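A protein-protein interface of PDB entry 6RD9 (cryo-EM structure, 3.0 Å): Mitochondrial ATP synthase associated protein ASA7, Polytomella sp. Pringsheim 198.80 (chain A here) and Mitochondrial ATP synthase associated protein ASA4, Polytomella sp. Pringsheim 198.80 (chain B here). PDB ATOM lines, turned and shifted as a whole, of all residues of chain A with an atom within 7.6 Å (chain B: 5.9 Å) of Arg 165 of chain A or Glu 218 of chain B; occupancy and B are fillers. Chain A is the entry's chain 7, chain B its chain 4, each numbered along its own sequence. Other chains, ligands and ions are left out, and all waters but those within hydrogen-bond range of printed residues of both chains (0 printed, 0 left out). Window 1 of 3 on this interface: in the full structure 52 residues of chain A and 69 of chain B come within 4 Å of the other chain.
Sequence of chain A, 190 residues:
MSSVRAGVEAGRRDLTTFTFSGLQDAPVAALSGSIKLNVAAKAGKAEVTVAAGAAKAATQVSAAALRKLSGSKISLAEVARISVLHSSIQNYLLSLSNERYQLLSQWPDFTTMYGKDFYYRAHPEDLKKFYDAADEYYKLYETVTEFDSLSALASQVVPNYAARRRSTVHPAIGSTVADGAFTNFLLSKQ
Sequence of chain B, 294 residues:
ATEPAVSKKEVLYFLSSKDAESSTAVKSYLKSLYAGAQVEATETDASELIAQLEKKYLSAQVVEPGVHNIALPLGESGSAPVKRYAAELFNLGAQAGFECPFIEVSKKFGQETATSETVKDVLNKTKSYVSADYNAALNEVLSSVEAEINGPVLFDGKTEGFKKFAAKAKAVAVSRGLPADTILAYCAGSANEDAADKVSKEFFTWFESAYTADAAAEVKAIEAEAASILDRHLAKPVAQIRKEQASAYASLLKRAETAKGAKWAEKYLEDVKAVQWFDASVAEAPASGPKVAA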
ATOM      1  N   LEU A  85     -27.201  13.100  10.771  1.00  0.00           N
ATOM      2  CA  LEU A  85     -26.879  14.031  11.839  1.00  0.00           C
ATOM      3  C   LEU A  85     -27.691  15.300  11.714  1.00  0.00           C
ATOM      4  O   LEU A  85     -28.294  15.755  12.684  1.00  0.00           O
ATOM      5  CB  LEU A  85     -25.401  14.362  11.807  1.00  0.00           C
ATOM      6  CG  LEU A  85     -24.986  15.531  12.667  1.00  0.00           C
ATOM      7  CD1 LEU A  85     -25.068  15.123  14.058  1.00  0.00           C
ATOM      8  CD2 LEU A  85     -23.612  15.941  12.340  1.00  0.00           C
ATOM      9  N   PRO A 159     -21.242  22.138  11.949  1.00  0.00           N
ATOM     10  CA  PRO A 159     -19.784  22.163  11.753  1.00  0.00           C
ATOM     11  C   PRO A 159     -18.971  22.311  13.016  1.00  0.00           C
ATOM     12  O   PRO A 159     -17.829  21.851  13.042  1.00  0.00           O
ATOM     13  CB  PRO A 159     -19.576  23.369  10.835  1.00  0.00           C
ATOM     14  CG  PRO A 159     -20.868  23.709  10.347  1.00  0.00           C
ATOM     15  CD  PRO A 159     -21.792  23.393  11.420  1.00  0.00           C
ATOM     16  N   ASN A 160     -19.501  22.945  14.052  1.00  0.00           N
ATOM     17  CA  ASN A 160     -18.795  23.004  15.323  1.00  0.00           C
ATOM     18  C   ASN A 160     -18.892  21.699  16.083  1.00  0.00           C
ATOM     19  O   ASN A 160     -17.978  21.362  16.834  1.00  0.00           O
ATOM     20  CB  ASN A 160     -19.348  24.130  16.182  1.00  0.00           C
ATOM     21  CG  ASN A 160     -18.723  25.452  15.867  1.00  0.00           C
ATOM     22  OD1 ASN A 160     -17.612  25.517  15.356  1.00  0.00           O
ATOM     23  ND2 ASN A 160     -19.427  26.522  16.173  1.00  0.00           N
ATOM     24  N   TYR A 161     -19.995  20.971  15.929  1.00  0.00           N
ATOM     25  CA  TYR A 161     -20.098  19.648  16.524  1.00  0.00           C
ATOM     26  C   TYR A 161     -19.164  18.682  15.829  1.00  0.00           C
ATOM     27  O   TYR A 161     -18.509  17.869  16.479  1.00  0.00           O
ATOM     28  CB  TYR A 161     -21.534  19.138  16.438  1.00  0.00           C
ATOM     29  CG  TYR A 161     -21.698  17.662  16.693  1.00  0.00           C
ATOM     30  CD1 TYR A 161     -21.812  16.765  15.650  1.00  0.00           C
ATOM     31  CD2 TYR A 161     -21.775  17.172  17.970  1.00  0.00           C
ATOM     32  CE1 TYR A 161     -21.944  15.441  15.877  1.00  0.00           C
ATOM     33  CE2 TYR A 161     -21.930  15.841  18.198  1.00  0.00           C
ATOM     34  CZ  TYR A 161     -22.010  14.986  17.146  1.00  0.00           C
ATOM     35  OH  TYR A 161     -22.170  13.650  17.351  1.00  0.00           O
ATOM     36  N   ALA A 162     -19.110  18.743  14.506  1.00  0.00           N
ATOM     37  CA  ALA A 162     -18.317  17.798  13.745  1.00  0.00           C
ATOM     38  C   ALA A 162     -16.829  17.998  13.936  1.00  0.00           C
ATOM     39  O   ALA A 162     -16.069  17.059  13.713  1.00  0.00           O
ATOM     40  CB  ALA A 162     -18.660  17.904  12.270  1.00  0.00           C
ATOM     41  N   ALA A 163     -16.397  19.183  14.349  1.00  0.00           N
ATOM     42  CA  ALA A 163     -14.992  19.410  14.638  1.00  0.00           C
ATOM     43  C   ALA A 163     -14.608  18.913  16.016  1.00  0.00           C
ATOM     44  O   ALA A 163     -13.446  18.589  16.246  1.00  0.00           O
ATOM     45  CB  ALA A 163     -14.666  20.888  14.514  1.00  0.00           C
ATOM     46  N   ARG A 164     -15.554  18.852  16.944  1.00  0.00           N
ATOM     47  CA  ARG A 164     -15.271  18.245  18.233  1.00  0.00           C
ATOM     48  C   ARG A 164     -15.180  16.742  18.125  1.00  0.00           C
ATOM     49  O   ARG A 164     -14.588  16.094  18.987  1.00  0.00           O
ATOM     50  CB  ARG A 164     -16.341  18.618  19.237  1.00  0.00           C
ATOM     51  CG  ARG A 164     -16.283  20.039  19.655  1.00  0.00           C
ATOM     52  CD  ARG A 164     -17.358  20.321  20.648  1.00  0.00           C
ATOM     53  NE  ARG A 164     -17.460  19.258  21.628  1.00  0.00           N
ATOM     54  CZ  ARG A 164     -16.760  19.225  22.748  1.00  0.00           C
ATOM     55  NH1 ARG A 164     -16.912  18.222  23.590  1.00  0.00           N
ATOM     56  NH2 ARG A 164     -15.907  20.193  23.024  1.00  0.00           N
ATOM     57  N   ARG A 165     -15.784  16.169  17.095  1.00  0.00           N
ATOM     58  CA  ARG A 165     -15.681  14.744  16.868  1.00  0.00           C
ATOM     59  C   ARG A 165     -14.430  14.377  16.107  1.00  0.00           C
ATOM     60  O   ARG A 165     -14.048  13.211  16.103  1.00  0.00           O
ATOM     61  CB  ARG A 165     -16.884  14.241  16.100  1.00  0.00           C
ATOM     62  CG  ARG A 165     -18.184  14.239  16.826  1.00  0.00           C
ATOM     63  CD  ARG A 165     -18.095  13.536  18.106  1.00  0.00           C
ATOM     64  NE  ARG A 165     -18.118  14.505  19.172  1.00  0.00           N
ATOM     65  CZ  ARG A 165     -18.005  14.198  20.446  1.00  0.00           C
ATOM     66  NH1 ARG A 165     -18.031  15.150  21.353  1.00  0.00           N
ATOM     67  NH2 ARG A 165     -17.863  12.941  20.806  1.00  0.00           N
ATOM     68  N   ARG A 166     -13.776  15.338  15.474  1.00  0.00           N
ATOM     69  CA  ARG A 166     -12.476  15.111  14.860  1.00  0.00           C
ATOM     70  C   ARG A 166     -11.369  15.308  15.871  1.00  0.00           C
ATOM     71  O   ARG A 166     -10.430  16.053  15.661  1.00  0.00           O
ATOM     72  CB  ARG A 166     -12.286  16.032  13.671  1.00  0.00           C
ATOM     73  CG  ARG A 166     -12.850  15.492  12.407  1.00  0.00           C
ATOM     74  CD  ARG A 166     -12.339  16.275  11.241  1.00  0.00           C
ATOM     75  NE  ARG A 166     -12.446  17.706  11.463  1.00  0.00           N
ATOM     76  CZ  ARG A 166     -13.527  18.422  11.196  1.00  0.00           C
ATOM     77  NH1 ARG A 166     -13.534  19.720  11.424  1.00  0.00           N
ATOM     78  NH2 ARG A 166     -14.598  17.845  10.703  1.00  0.00           N
ATOM     79  N   SER A 167     -11.486  14.620  16.991  1.00  0.00           N
ATOM     80  CA  SER A 167     -10.513  14.727  18.048  1.00  0.00           C
ATOM     81  C   SER A 167      -9.316  13.878  17.690  1.00  0.00           C
ATOM     82  O   SER A 167      -9.435  12.870  17.001  1.00  0.00           O
ATOM     83  CB  SER A 167     -11.125  14.275  19.365  1.00  0.00           C
ATOM     84  OG  SER A 167     -10.238  14.454  20.439  1.00  0.00           O
ATOM     85  N   THR A 168      -8.151  14.306  18.141  1.00  0.00           N
ATOM     86  CA  THR A 168      -6.936  13.548  17.909  1.00  0.00           C
ATOM     87  C   THR A 168      -6.785  12.385  18.869  1.00  0.00           C
ATOM     88  O   THR A 168      -5.831  11.618  18.741  1.00  0.00           O
ATOM     89  CB  THR A 168      -5.730  14.461  18.035  1.00  0.00           C
ATOM     90  OG1 THR A 168      -5.688  14.994  19.360  1.00  0.00           O
ATOM     91  CG2 THR A 168      -5.842  15.589  17.061  1.00  0.00           C
ATOM     92  N   VAL A 169      -7.695  12.237  19.823  1.00  0.00           N
ATOM     93  CA  VAL A 169      -7.646  11.149  20.782  1.00  0.00           C
ATOM     94  C   VAL A 169      -8.628  10.068  20.366  1.00  0.00           C
ATOM     95  O   VAL A 169      -8.228   8.937  20.092  1.00  0.00           O
ATOM     96  CB  VAL A 169      -7.945  11.661  22.192  1.00  0.00           C
ATOM     97  CG1 VAL A 169      -7.948  10.541  23.152  1.00  0.00           C
ATOM     98  CG2 VAL A 169      -6.920  12.653  22.588  1.00  0.00           C
ATOM     99  N   HIS A 170      -9.910  10.408  20.300  1.00  0.00           N
ATOM    100  CA  HIS A 170     -10.970   9.476  19.944  1.00  0.00           C
ATOM    101  C   HIS A 170     -12.207  10.285  19.617  1.00  0.00           C
ATOM    102  O   HIS A 170     -12.374  11.379  20.158  1.00  0.00           O
ATOM    103  CB  HIS A 170     -11.261   8.501  21.090  1.00  0.00           C
ATOM    104  CG  HIS A 170     -12.029   7.289  20.676  1.00  0.00           C
ATOM    105  ND1 HIS A 170     -11.425   6.112  20.317  1.00  0.00           N
ATOM    106  CD2 HIS A 170     -13.356   7.070  20.578  1.00  0.00           C
ATOM    107  CE1 HIS A 170     -12.348   5.225  20.003  1.00  0.00           C
ATOM    108  NE2 HIS A 170     -13.529   5.783  20.151  1.00  0.00           N
ATOM    109  N   PRO A 171     -13.077   9.800  18.727  1.00  0.00           N
ATOM    110  CA  PRO A 171     -14.360  10.480  18.511  1.00  0.00           C
ATOM    111  C   PRO A 171     -15.260  10.530  19.726  1.00  0.00           C
ATOM    112  O   PRO A 171     -15.990  11.505  19.899  1.00  0.00           O
ATOM    113  CB  PRO A 171     -14.996   9.645  17.406  1.00  0.00           C
ATOM    114  CG  PRO A 171     -13.889   9.072  16.708  1.00  0.00           C
ATOM    115  CD  PRO A 171     -12.791   8.850  17.649  1.00  0.00           C
ATOM    116  N   ALA A 172     -15.221   9.512  20.579  1.00  0.00           N
ATOM    117  CA  ALA A 172     -16.106   9.368  21.717  1.00  0.00           C
ATOM    118  C   ALA A 172     -15.458   9.755  23.027  1.00  0.00           C
ATOM    119  O   ALA A 172     -15.961   9.379  24.085  1.00  0.00           O
ATOM    120  CB  ALA A 172     -16.602   7.933  21.813  1.00  0.00           C
ATOM    121  N   ILE A 173     -14.370  10.474  22.993  1.00  0.00           N
ATOM    122  CA  ILE A 173     -13.681  10.822  24.225  1.00  0.00           C
ATOM    123  C   ILE A 173     -14.436  11.946  24.917  1.00  0.00           C
ATOM    124  O   ILE A 173     -15.151  12.730  24.288  1.00  0.00           O
ATOM    125  CB  ILE A 173     -12.212  11.186  23.931  1.00  0.00           C
ATOM    126  CG1 ILE A 173     -11.336  11.022  25.169  1.00  0.00           C
ATOM    127  CG2 ILE A 173     -12.080  12.570  23.349  1.00  0.00           C
ATOM    128  CD1 ILE A 173     -11.401   9.688  25.789  1.00  0.00           C
ATOM    129  N   GLY A 174     -14.339  11.984  26.241  1.00  0.00           N
ATOM    130  CA  GLY A 174     -14.909  13.062  27.015  1.00  0.00           C
ATOM    131  C   GLY A 174     -14.085  13.291  28.259  1.00  0.00           C
ATOM    132  O   GLY A 174     -13.052  12.665  28.448  1.00  0.00           O
ATOM    133  N   VAL B  63     -13.837   8.943  10.129  1.00  0.00           N
ATOM    134  CA  VAL B  63     -14.615   9.554  11.195  1.00  0.00           C
ATOM    135  C   VAL B  63     -15.564  10.600  10.633  1.00  0.00           C
ATOM    136  O   VAL B  63     -16.733  10.660  11.018  1.00  0.00           O
ATOM    137  CB  VAL B  63     -13.669  10.132  12.256  1.00  0.00           C
ATOM    138  CG1 VAL B  63     -14.357  11.132  13.120  1.00  0.00           C
ATOM    139  CG2 VAL B  63     -13.152   9.034  13.094  1.00  0.00           C
ATOM    140  N   VAL B  67     -19.491  10.501  11.430  1.00  0.00           N
ATOM    141  CA  VAL B  67     -20.125  11.360  12.421  1.00  0.00           C
ATOM    142  C   VAL B  67     -21.427  11.910  11.877  1.00  0.00           C
ATOM    143  O   VAL B  67     -22.424  12.031  12.595  1.00  0.00           O
ATOM    144  CB  VAL B  67     -19.143  12.469  12.817  1.00  0.00           C
ATOM    145  CG1 VAL B  67     -19.816  13.607  13.502  1.00  0.00           C
ATOM    146  CG2 VAL B  67     -18.148  11.880  13.715  1.00  0.00           C
ATOM    147  N   LEU B  72     -27.891  12.329  16.457  1.00  0.00           N
ATOM    148  CA  LEU B  72     -27.814  12.789  17.827  1.00  0.00           C
ATOM    149  C   LEU B  72     -29.123  12.489  18.548  1.00  0.00           C
ATOM    150  O   LEU B  72     -30.193  12.593  17.953  1.00  0.00           O
ATOM    151  CB  LEU B  72     -27.555  14.278  17.848  1.00  0.00           C
ATOM    152  CG  LEU B  72     -26.138  14.779  17.861  1.00  0.00           C
ATOM    153  CD1 LEU B  72     -26.157  16.168  17.403  1.00  0.00           C
ATOM    154  CD2 LEU B  72     -25.683  14.755  19.259  1.00  0.00           C
ATOM    155  N   LEU B  74     -31.092  14.107  20.486  1.00  0.00           N
ATOM    156  CA  LEU B  74     -31.478  15.384  21.050  1.00  0.00           C
ATOM    157  C   LEU B  74     -32.916  15.332  21.517  1.00  0.00           C
ATOM    158  O   LEU B  74     -33.794  14.861  20.791  1.00  0.00           O
ATOM    159  CB  LEU B  74     -31.307  16.484  20.021  1.00  0.00           C
ATOM    160  CG  LEU B  74     -29.922  16.651  19.467  1.00  0.00           C
ATOM    161  CD1 LEU B  74     -29.916  17.713  18.461  1.00  0.00           C
ATOM    162  CD2 LEU B  74     -29.055  17.046  20.582  1.00  0.00           C
ATOM    163  N   TYR B  85     -25.979   6.417  21.119  1.00  0.00           N
ATOM    164  CA  TYR B  85     -25.167   7.439  20.490  1.00  0.00           C
ATOM    165  C   TYR B  85     -23.720   7.279  20.861  1.00  0.00           C
ATOM    166  O   TYR B  85     -22.841   7.523  20.038  1.00  0.00           O
ATOM    167  CB  TYR B  85     -25.659   8.810  20.901  1.00  0.00           C
ATOM    168  CG  TYR B  85     -24.735   9.911  20.545  1.00  0.00           C
ATOM    169  CD1 TYR B  85     -24.143  10.666  21.513  1.00  0.00           C
ATOM    170  CD2 TYR B  85     -24.455  10.193  19.237  1.00  0.00           C
ATOM    171  CE1 TYR B  85     -23.301  11.667  21.191  1.00  0.00           C
ATOM    172  CE2 TYR B  85     -23.615  11.184  18.907  1.00  0.00           C
ATOM    173  CZ  TYR B  85     -23.040  11.915  19.891  1.00  0.00           C
ATOM    174  OH  TYR B  85     -22.188  12.926  19.577  1.00  0.00           O
ATOM    175  N   LEU B  89     -20.356   5.883  18.294  1.00  0.00           N
ATOM    176  CA  LEU B  89     -19.083   6.577  18.239  1.00  0.00           C
ATOM    177  C   LEU B  89     -17.928   5.713  18.699  1.00  0.00           C
ATOM    178  O   LEU B  89     -16.797   5.968  18.303  1.00  0.00           O
ATOM    179  CB  LEU B  89     -19.130   7.824  19.103  1.00  0.00           C
ATOM    180  CG  LEU B  89     -19.940   9.051  18.741  1.00  0.00           C
ATOM    181  CD1 LEU B  89     -19.878   9.973  19.902  1.00  0.00           C
ATOM    182  CD2 LEU B  89     -19.367   9.711  17.542  1.00  0.00           C
ATOM    183  N   ALA B 213     -22.027   9.840  30.385  1.00  0.00           N
ATOM    184  CA  ALA B 213     -22.018  11.209  30.860  1.00  0.00           C
ATOM    185  C   ALA B 213     -21.163  12.128  30.011  1.00  0.00           C
ATOM    186  O   ALA B 213     -21.240  13.339  30.189  1.00  0.00           O
ATOM    187  CB  ALA B 213     -21.540  11.255  32.298  1.00  0.00           C
ATOM    188  N   ASP B 214     -20.332  11.607  29.121  1.00  0.00           N
ATOM    189  CA  ASP B 214     -19.696  12.494  28.159  1.00  0.00           C
ATOM    190  C   ASP B 214     -20.531  12.656  26.912  1.00  0.00           C
ATOM    191  O   ASP B 214     -20.472  13.703  26.268  1.00  0.00           O
ATOM    192  CB  ASP B 214     -18.330  11.990  27.728  1.00  0.00           C
ATOM    193  CG  ASP B 214     -17.465  11.581  28.866  1.00  0.00           C
ATOM    194  OD1 ASP B 214     -17.200  10.378  28.996  1.00  0.00           O
ATOM    195  OD2 ASP B 214     -17.043  12.464  29.632  1.00  0.00           O
ATOM    196  N   ALA B 215     -21.263  11.620  26.525  1.00  0.00           N
ATOM    197  CA  ALA B 215     -22.193  11.758  25.422  1.00  0.00           C
ATOM    198  C   ALA B 215     -23.377  12.608  25.828  1.00  0.00           C
ATOM    199  O   ALA B 215     -23.821  13.457  25.057  1.00  0.00           O
ATOM    200  CB  ALA B 215     -22.658  10.392  24.951  1.00  0.00           C
ATOM    201  N   ALA B 216     -23.880  12.423  27.044  1.00  0.00           N
ATOM    202  CA  ALA B 216     -25.029  13.198  27.484  1.00  0.00           C
ATOM    203  C   ALA B 216     -24.663  14.639  27.751  1.00  0.00           C
ATOM    204  O   ALA B 216     -25.526  15.506  27.686  1.00  0.00           O
ATOM    205  CB  ALA B 216     -25.651  12.587  28.729  1.00  0.00           C
ATOM    206  N   ALA B 217     -23.407  14.920  28.059  1.00  0.00           N
ATOM    207  CA  ALA B 217     -22.977  16.303  28.150  1.00  0.00           C
ATOM    208  C   ALA B 217     -22.760  16.916  26.787  1.00  0.00           C
ATOM    209  O   ALA B 217     -22.737  18.139  26.671  1.00  0.00           O
ATOM    210  CB  ALA B 217     -21.695  16.412  28.954  1.00  0.00           C
ATOM    211  N   GLU B 218     -22.552  16.097  25.766  1.00  0.00           N
ATOM    212  CA  GLU B 218     -22.430  16.597  24.408  1.00  0.00           C
ATOM    213  C   GLU B 218     -23.788  16.867  23.801  1.00  0.00           C
ATOM    214  O   GLU B 218     -23.940  17.800  23.017  1.00  0.00           O
ATOM    215  CB  GLU B 218     -21.666  15.587  23.561  1.00  0.00           C
ATOM    216  CG  GLU B 218     -21.304  16.075  22.200  1.00  0.00           C
ATOM    217  CD  GLU B 218     -20.324  17.217  22.244  1.00  0.00           C
ATOM    218  OE1 GLU B 218     -19.183  16.990  22.702  1.00  0.00           O
ATOM    219  OE2 GLU B 218     -20.696  18.338  21.827  1.00  0.00           O
ATOM    220  N   VAL B 219     -24.775  16.053  24.151  1.00  0.00           N
ATOM    221  CA  VAL B 219     -26.142  16.264  23.708  1.00  0.00           C
ATOM    222  C   VAL B 219     -26.739  17.479  24.390  1.00  0.00           C
ATOM    223  O   VAL B 219     -27.386  18.302  23.748  1.00  0.00           O
ATOM    224  CB  VAL B 219     -26.952  14.992  23.984  1.00  0.00           C
ATOM    225  CG1 VAL B 219     -28.405  15.216  23.797  1.00  0.00           C
ATOM    226  CG2 VAL B 219     -26.469  13.911  23.104  1.00  0.00           C
ATOM    227  N   LYS B 220     -26.478  17.653  25.683  1.00  0.00           N
ATOM    228  CA  LYS B 220     -27.005  18.805  26.402  1.00  0.00           C
ATOM    229  C   LYS B 220     -26.343  20.107  26.003  1.00  0.00           C
ATOM    230  O   LYS B 220     -26.815  21.162  26.413  1.00  0.00           O
ATOM    231  CB  LYS B 220     -26.852  18.623  27.904  1.00  0.00           C
ATOM    232  CG  LYS B 220     -27.818  17.643  28.506  1.00  0.00           C
ATOM    233  CD  LYS B 220     -29.252  18.019  28.226  1.00  0.00           C
ATOM    234  CE  LYS B 220     -30.189  16.893  28.617  1.00  0.00           C
ATOM    235  NZ  LYS B 220     -31.612  17.294  28.526  1.00  0.00           N
ATOM    236  N   ALA B 221     -25.262  20.069  25.248  1.00  0.00           N
ATOM    237  CA  ALA B 221     -24.697  21.288  24.710  1.00  0.00           C
ATOM    238  C   ALA B 221     -25.171  21.580  23.309  1.00  0.00           C
ATOM    239  O   ALA B 221     -25.149  22.735  22.893  1.00  0.00           O
ATOM    240  CB  ALA B 221     -23.183  21.210  24.702  1.00  0.00           C
ATOM    241  N   ILE B 222     -25.551  20.555  22.554  1.00  0.00           N
ATOM    242  CA  ILE B 222     -26.162  20.768  21.250  1.00  0.00           C
ATOM    243  C   ILE B 222     -27.605  21.193  21.421  1.00  0.00           C
ATOM    244  O   ILE B 222     -28.113  22.029  20.675  1.00  0.00           O
ATOM    245  CB  ILE B 222     -26.032  19.492  20.399  1.00  0.00           C
ATOM    246  CG1 ILE B 222     -24.577  19.200  20.107  1.00  0.00           C
ATOM    247  CG2 ILE B 222     -26.727  19.625  19.097  1.00  0.00           C
ATOM    248  CD1 ILE B 222     -23.880  20.309  19.408  1.00  0.00           C
ATOM    249  N   GLU B 223     -28.277  20.647  22.427  1.00  0.00           N
ATOM    250  CA  GLU B 223     -29.623  21.079  22.761  1.00  0.00           C
ATOM    251  C   GLU B 223     -29.643  22.521  23.219  1.00  0.00           C
ATOM    252  O   GLU B 223     -30.574  23.262  22.912  1.00  0.00           O
ATOM    253  CB  GLU B 223     -30.185  20.203  23.861  1.00  0.00           C
ATOM    254  CG  GLU B 223     -30.604  18.858  23.431  1.00  0.00           C
ATOM    255  CD  GLU B 223     -31.215  18.101  24.556  1.00  0.00           C
ATOM    256  OE1 GLU B 223     -31.429  18.713  25.610  1.00  0.00           O
ATOM    257  OE2 GLU B 223     -31.489  16.902  24.402  1.00  0.00           O
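Hydrophobic or aromatic side chains of chain A within 4 Å of the printed part of chain B: Leu 85, Tyr 161, His 170, Pro 171 and Ala 172.
The guanidinium group (NH2) of Arg 165 of chain A is in hydrogen-bond range of the backbone carbonyl oxygen (O) of Pro 171 of chain A (2.5 Å).
Val 67 of chain B touches Leu 85 of chain A. CD1 of Leu 85 of chain A touches CD1 of Leu 72 of chain B, at 3.7 Å. Ile 222 of chain B touches Tyr 161 of chain A. Arg 165 of chain A touches Val 63 of chain B (O to CG1, 3.6 Å). CB of Arg 165 of chain A touches CG2 of Val 67 of chain B, at 3.6 Å. Arg 165 of chain A touches Leu 89 of chain B. His 170 of chain A touches Leu 89 of chain B. Pro 171 of chain A touches Val 63 of chain B (CG to CG2, 3.7 Å). Ala 172 of chain A touches Leu 89 of chain B (CB to CB, 3.7 Å). C of Gly 174 of chain A touches OD2 of Asp 214 of chain B, 3.4 Å away.
OE1 of Glu 218 of chain B is in salt-bridge range of NH1 of Arg 164 of chain A, 2.7 Å away. The side-chain carboxylate (OE1) of Glu 218 of chain B lies within salt-bridge range of the guanidinium group (NH1) of Arg 165 of chain A. The side-chain hydroxyl of Tyr 161 of chain A sits close to the side-chain hydroxyl of Tyr 85 of chain B, 2.3 Å away.
No residue of chain A comes within 4 Å of Ala 217 of chain B. Of the printed residues of chain B, Pro 171 of chain A touches Val 63. Of the printed residues of chain B, Leu 85 of chain A touches Val 67 and Leu 72. Ala 216 of chain B touches none of the printed residues of chain A. Leu 74 of chain B touches none of the printed residues of chain A. The nearest residue of chain A that does not touch Glu 218 of chain B is Tyr 161 of chain A (4.1 Å). The nearest printed residue of chain A that does not touch Asp 214 of chain B is Ile 173 of chain A (4.7 Å).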
